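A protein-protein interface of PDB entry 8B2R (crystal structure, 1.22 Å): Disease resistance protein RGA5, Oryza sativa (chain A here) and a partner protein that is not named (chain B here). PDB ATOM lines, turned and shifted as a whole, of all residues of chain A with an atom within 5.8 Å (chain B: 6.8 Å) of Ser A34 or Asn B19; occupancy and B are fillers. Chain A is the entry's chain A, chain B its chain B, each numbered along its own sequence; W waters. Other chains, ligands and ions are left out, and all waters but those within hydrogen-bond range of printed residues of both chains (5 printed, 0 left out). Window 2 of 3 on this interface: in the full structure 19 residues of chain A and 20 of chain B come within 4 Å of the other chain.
The side-chain hydroxyl (OG) of Ser A34 lies within hydrogen-bond range of the side-chain amide nitrogen (ND2) of Asn B19.
The side-chain amide nitrogen of Asn B19 is in hydrogen-bond range of the side-chain carboxylate of Glu A36.
The backbone carbonyl oxygen (O) of Phe B17 lies within hydrogen-bond range of the side-chain amide nitrogen (NE2) of Gln A46 (3.0 Å).
The backbone carbonyl oxygen (O) of Val A48 is in hydrogen-bond range of the backbone NH (N) of Asp A33 (2.8 Å).
The backbone NH of Val A48 sits at hydrogen-bond distance from the backbone carbonyl oxygen of Ser A34 (3.1 Å).
The backbone carbonyl oxygen (O) of Glu A36 sits at hydrogen-bond distance from the backbone NH (N) of Gln A46, 2.7 Å away.
The backbone NH of Asp B21 is in hydrogen-bond range of the side-chain amide oxygen of Asn B19, 2.8 Å away.
The side-chain amide oxygen (OD1) of Asn B19 lies within hydrogen-bond range of the backbone NH (N) of Ile B22 (3.5 Å).
Among the printed residues, merely in contact across the chains: Glu A36 with Phe B17 and Val A48 with Ile B22.
Of chain B, only Asn B19 comes within 4 Å of Ser A34.
Printed residues of chain B within 4 Å of Glu A36: Phe B17 (3.2 Å) and Asn B19 (3.2 Å).
Printed residues of chain B within 4 Å of Val A48: Ile B22.
Of the printed residues of chain A, Phe B17 touches Glu A36 (3.2 Å) and Gln A46 (3.0 Å).
Printed residues of chain A within 4 Å of Ile B22: Val A48 (3.8 Å).
Printed residues of chain B within 4 Å of Gln A46: Phe B17 (3.0 Å).
The nearest residue of chain B that does not touch Ser A34 is Asp B21 (4.4 Å).
The nearest printed residue of chain B that does not touch Val A48 is Asn B19 (4.2 Å).
Printed residues of chain A that touch a printed residue of chain B: Ser A34, Glu A36, Gln A46 and Val A48.
Of the 9 printed residues of chain B, 3 touch a printed residue of chain A.
Hydrophobic or aromatic side chains of chain B that line the printed part of chain A: Phe B17 and Ile B22.
Among the printed residues, 5 pairs touch across the chains.
Among the printed residues, no Asp or Glu carboxylate lies within 4 Å of a Lys or Arg side-chain nitrogen of the other chain.
Water W3 lies within hydrogen-bond range of OE1 of Gln A46 and O of Phe B17.
Water W1 bridges the side-chain amide oxygen of Gln A46 (2.6 Å) and the backbone NH of Phe B17 (2.8 Å).
Water W5 lies within hydrogen-bond range of the side-chain carboxylate (OE1) of Glu A36 (2.7 Å), the side-chain hydroxyl (OG) of Ser A34 (2.8 Å), the backbone carbonyl oxygen (O) of Gln A46 (2.9 Å) and the side-chain amide nitrogen (ND2) of Asn B19 (3.5 Å).
Water W4 lies within hydrogen-bond range of the side-chain carboxylate of Asp B21, the side-chain hydroxyl of Ser A34 and the side-chain amide oxygen of Asn B19.
Water W2 bridges OE2 of Glu A36 (2.8 Å) and N of Ala B20 (3.0 Å).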
ATOM      1  N   VAL A  32     -10.109  15.586  31.122  1.00  0.00           N
ATOM      2  CA  VAL A  32     -10.981  16.624  30.617  1.00  0.00           C
ATOM      3  C   VAL A  32     -10.285  17.430  29.526  1.00  0.00           C
ATOM      4  O   VAL A  32      -9.169  17.946  29.677  1.00  0.00           O
ATOM      5  CB  VAL A  32     -11.453  17.520  31.784  1.00  0.00           C
ATOM      6  CG1 VAL A  32     -12.208  18.756  31.287  1.00  0.00           C
ATOM      7  CG2 VAL A  32     -12.284  16.731  32.799  1.00  0.00           C
ATOM      8  N   ASP A  33     -10.962  17.574  28.390  1.00  0.00           N
ATOM      9  CA  ASP A  33     -10.465  18.337  27.267  1.00  0.00           C
ATOM     10  C   ASP A  33     -11.170  19.688  27.137  1.00  0.00           C
ATOM     11  O   ASP A  33     -10.613  20.658  26.632  1.00  0.00           O
ATOM     12  CB  ASP A  33     -10.659  17.544  25.982  1.00  0.00           C
ATOM     13  CG  ASP A  33      -9.744  16.329  25.908  1.00  0.00           C
ATOM     14  OD1 ASP A  33      -8.669  16.339  26.493  1.00  0.00           O
ATOM     15  OD2 ASP A  33     -10.126  15.409  25.255  1.00  0.00           O
ATOM     16  N   SER A  34     -12.420  19.808  27.566  1.00  0.00           N
ATOM     17  CA  SER A  34     -13.143  21.053  27.447  1.00  0.00           C
ATOM     18  C   SER A  34     -14.222  21.105  28.509  1.00  0.00           C
ATOM     19  O   SER A  34     -14.711  20.053  28.925  1.00  0.00           O
ATOM     20  CB  SER A  34     -13.770  21.234  26.077  1.00  0.00           C
ATOM     21  OG  SER A  34     -14.710  20.261  25.812  1.00  0.00           O
ATOM     22  N   VAL A  35     -14.546  22.348  28.913  1.00  0.00           N
ATOM     23  CA  VAL A  35     -15.553  22.612  29.909  1.00  0.00           C
ATOM     24  C   VAL A  35     -16.318  23.842  29.449  1.00  0.00           C
ATOM     25  O   VAL A  35     -15.709  24.889  29.172  1.00  0.00           O
ATOM     26  CB  VAL A  35     -14.978  22.901  31.310  1.00  0.00           C
ATOM     27  CG1 VAL A  35     -16.067  22.922  32.366  1.00  0.00           C
ATOM     28  CG2 VAL A  35     -13.867  21.943  31.687  1.00  0.00           C
ATOM     29  N   GLU A  36     -17.632  23.715  29.380  1.00  0.00           N
ATOM     30  CA  GLU A  36     -18.474  24.843  29.036  1.00  0.00           C
ATOM     31  C   GLU A  36     -19.667  24.891  29.981  1.00  0.00           C
ATOM     32  O   GLU A  36     -20.109  23.888  30.482  1.00  0.00           O
ATOM     33  CB  GLU A  36     -18.995  24.673  27.605  1.00  0.00           C
ATOM     34  CG  GLU A  36     -17.886  24.685  26.570  1.00  0.00           C
ATOM     35  CD  GLU A  36     -17.983  23.725  25.401  1.00  0.00           C
ATOM     36  OE1 GLU A  36     -18.612  22.620  25.472  1.00  0.00           O
ATOM     37  OE2 GLU A  36     -17.427  24.102  24.385  1.00  0.00           O
ATOM     38  N   GLN A  46     -20.833  21.303  31.036  1.00  0.00           N
ATOM     39  CA  GLN A  46     -20.680  20.320  29.943  1.00  0.00           C
ATOM     40  C   GLN A  46     -19.189  20.060  29.784  1.00  0.00           C
ATOM     41  O   GLN A  46     -18.425  20.976  29.522  1.00  0.00           O
ATOM     42  CB  GLN A  46     -21.243  20.914  28.628  1.00  0.00           C
ATOM     43  CG  GLN A  46     -21.055  20.080  27.356  1.00  0.00           C
ATOM     44  CD  GLN A  46     -21.892  20.676  26.252  1.00  0.00           C
ATOM     45  OE1 GLN A  46     -23.086  20.382  26.186  1.00  0.00           O
ATOM     46  NE2 GLN A  46     -21.320  21.471  25.365  1.00  0.00           N
ATOM     47  N   VAL A  47     -18.778  18.825  30.045  1.00  0.00           N
ATOM     48  CA  VAL A  47     -17.407  18.448  30.031  1.00  0.00           C
ATOM     49  C   VAL A  47     -17.237  17.373  28.953  1.00  0.00           C
ATOM     50  O   VAL A  47     -18.057  16.444  28.836  1.00  0.00           O
ATOM     51  CB  VAL A  47     -17.082  17.895  31.423  1.00  0.00           C
ATOM     52  CG1 VAL A  47     -15.696  17.333  31.443  1.00  0.00           C
ATOM     53  CG2 VAL A  47     -17.295  18.936  32.511  1.00  0.00           C
ATOM     54  N   VAL A  48     -16.162  17.470  28.171  1.00  0.00           N
ATOM     55  CA  VAL A  48     -15.844  16.454  27.210  1.00  0.00           C
ATOM     56  C   VAL A  48     -14.414  15.994  27.494  1.00  0.00           C
ATOM     57  O   VAL A  48     -13.534  16.795  27.785  1.00  0.00           O
ATOM     58  CB  VAL A  48     -15.910  16.999  25.778  1.00  0.00           C
ATOM     59  CG1 VAL A  48     -15.438  15.977  24.770  1.00  0.00           C
ATOM     60  CG2 VAL A  48     -17.320  17.445  25.457  1.00  0.00           C
ATOM     61  N   GLY A  49     -14.195  14.697  27.486  1.00  0.00           N
ATOM     62  CA  GLY A  49     -12.822  14.244  27.593  1.00  0.00           C
ATOM     63  C   GLY A  49     -12.734  12.728  27.461  1.00  0.00           C
ATOM     64  O   GLY A  49     -13.605  12.072  26.888  1.00  0.00           O
ATOM     65  N   PHE B  17     -25.230  23.846  23.668  1.00  0.00           N
ATOM     66  CA  PHE B  17     -24.023  24.305  23.014  1.00  0.00           C
ATOM     67  C   PHE B  17     -23.369  23.131  22.323  1.00  0.00           C
ATOM     68  O   PHE B  17     -23.003  22.173  22.985  1.00  0.00           O
ATOM     69  CB  PHE B  17     -23.048  24.954  24.012  1.00  0.00           C
ATOM     70  CG  PHE B  17     -21.880  25.628  23.323  1.00  0.00           C
ATOM     71  CD1 PHE B  17     -22.004  26.899  22.749  1.00  0.00           C
ATOM     72  CD2 PHE B  17     -20.656  24.972  23.214  1.00  0.00           C
ATOM     73  CE1 PHE B  17     -20.923  27.503  22.125  1.00  0.00           C
ATOM     74  CE2 PHE B  17     -19.575  25.579  22.581  1.00  0.00           C
ATOM     75  CZ  PHE B  17     -19.712  26.840  22.028  1.00  0.00           C
ATOM     76  N   ASP B  18     -23.202  23.269  21.020  1.00  0.00           N
ATOM     77  CA  ASP B  18     -22.531  22.228  20.244  1.00  0.00           C
ATOM     78  C   ASP B  18     -20.996  22.428  20.365  1.00  0.00           C
ATOM     79  O   ASP B  18     -20.418  23.308  19.768  1.00  0.00           O
ATOM     80  CB  ASP B  18     -22.946  22.286  18.773  1.00  0.00           C
ATOM     81  CG  ASP B  18     -24.412  21.935  18.538  1.00  0.00           C
ATOM     82  OD1 ASP B  18     -24.895  20.956  19.155  1.00  0.00           O
ATOM     83  OD2 ASP B  18     -25.039  22.614  17.685  1.00  0.00           O
ATOM     84  N   ASN B  19     -20.336  21.562  21.120  1.00  0.00           N
ATOM     85  CA  ASN B  19     -18.902  21.621  21.272  1.00  0.00           C
ATOM     86  C   ASN B  19     -18.215  21.487  19.925  1.00  0.00           C
ATOM     87  O   ASN B  19     -18.594  20.674  19.079  1.00  0.00           O
ATOM     88  CB  ASN B  19     -18.469  20.505  22.227  1.00  0.00           C
ATOM     89  CG  ASN B  19     -16.983  20.476  22.427  1.00  0.00           C
ATOM     90  OD1 ASN B  19     -16.247  19.858  21.652  1.00  0.00           O
ATOM     91  ND2 ASN B  19     -16.536  21.112  23.486  1.00  0.00           N
ATOM     92  N   ALA B  20     -17.185  22.300  19.707  1.00  0.00           N
ATOM     93  CA  ALA B  20     -16.577  22.413  18.402  1.00  0.00           C
ATOM     94  C   ALA B  20     -15.787  21.150  18.027  1.00  0.00           C
ATOM     95  O   ALA B  20     -15.485  20.957  16.846  1.00  0.00           O
ATOM     96  CB  ALA B  20     -15.653  23.618  18.367  1.00  0.00           C
ATOM     97  N   ASP B  21     -15.323  20.386  19.029  1.00  0.00           N
ATOM     98  CA  ASP B  21     -14.304  19.361  18.857  1.00  0.00           C
ATOM     99  C   ASP B  21     -14.878  17.945  18.729  1.00  0.00           C
ATOM    100  O   ASP B  21     -14.141  16.972  18.600  1.00  0.00           O
ATOM    101  CB  ASP B  21     -13.322  19.320  20.038  1.00  0.00           C
ATOM    102  CG  ASP B  21     -12.753  20.631  20.573  1.00  0.00           C
ATOM    103  OD1 ASP B  21     -12.323  21.401  19.744  1.00  0.00           O
ATOM    104  OD2 ASP B  21     -12.637  20.785  21.866  1.00  0.00           O
ATOM    105  N   ILE B  22     -16.204  17.817  18.820  1.00  0.00           N
ATOM    106  CA  ILE B  22     -16.909  16.539  18.695  1.00  0.00           C
ATOM    107  C   ILE B  22     -18.026  16.687  17.666  1.00  0.00           C
ATOM    108  O   ILE B  22     -18.490  17.791  17.405  1.00  0.00           O
ATOM    109  CB  ILE B  22     -17.468  16.047  20.044  1.00  0.00           C
ATOM    110  CG1 ILE B  22     -18.536  16.980  20.622  1.00  0.00           C
ATOM    111  CG2 ILE B  22     -16.388  15.801  21.063  1.00  0.00           C
ATOM    112  CD1 ILE B  22     -19.138  16.494  21.928  1.00  0.00           C
ATOM    113  N   PRO B  23     -18.479  15.563  17.050  1.00  0.00           N
ATOM    114  CA  PRO B  23     -19.519  15.669  16.035  1.00  0.00           C
ATOM    115  C   PRO B  23     -20.773  16.323  16.639  1.00  0.00           C
ATOM    116  O   PRO B  23     -21.095  16.170  17.819  1.00  0.00           O
ATOM    117  CB  PRO B  23     -19.743  14.221  15.588  1.00  0.00           C
ATOM    118  CG  PRO B  23     -18.426  13.587  15.817  1.00  0.00           C
ATOM    119  CD  PRO B  23     -17.941  14.181  17.128  1.00  0.00           C
ATOM    120  N   VAL B  24     -21.498  17.040  15.785  1.00  0.00           N
ATOM    121  CA  VAL B  24     -22.761  17.634  16.214  1.00  0.00           C
ATOM    122  C   VAL B  24     -23.808  16.551  16.442  1.00  0.00           C
ATOM    123  O   VAL B  24     -24.065  15.749  15.547  1.00  0.00           O
ATOM    124  CB  VAL B  24     -23.255  18.707  15.231  1.00  0.00           C
ATOM    125  CG1 VAL B  24     -24.518  19.371  15.719  1.00  0.00           C
ATOM    126  CG2 VAL B  24     -22.197  19.739  14.930  1.00  0.00           C
ATOM    127  N   PRO B  25     -24.423  16.500  17.646  1.00  0.00           N
ATOM    128  CA  PRO B  25     -25.452  15.513  17.894  1.00  0.00           C
ATOM    129  C   PRO B  25     -26.727  15.784  17.091  1.00  0.00           C
ATOM    130  O   PRO B  25     -27.111  16.919  16.945  1.00  0.00           O
ATOM    131  CB  PRO B  25     -25.658  15.529  19.401  1.00  0.00           C
ATOM    132  CG  PRO B  25     -25.289  16.964  19.764  1.00  0.00           C
ATOM    133  CD  PRO B  25     -24.116  17.289  18.842  1.00  0.00           C
HETATM  134  O   HOH W   1     -25.258  21.387  25.104  1.00  0.00           O
HETATM  135  O   HOH W   2     -16.549  24.339  21.754  1.00  0.00           O
HETATM  136  O   HOH W   3     -23.823  19.328  24.082  1.00  0.00           O
HETATM  137  O   HOH W   4     -13.637  18.892  23.613  1.00  0.00           O
HETATM  138  O   HOH W   5     -17.197  20.759  26.904  1.00  0.00           O
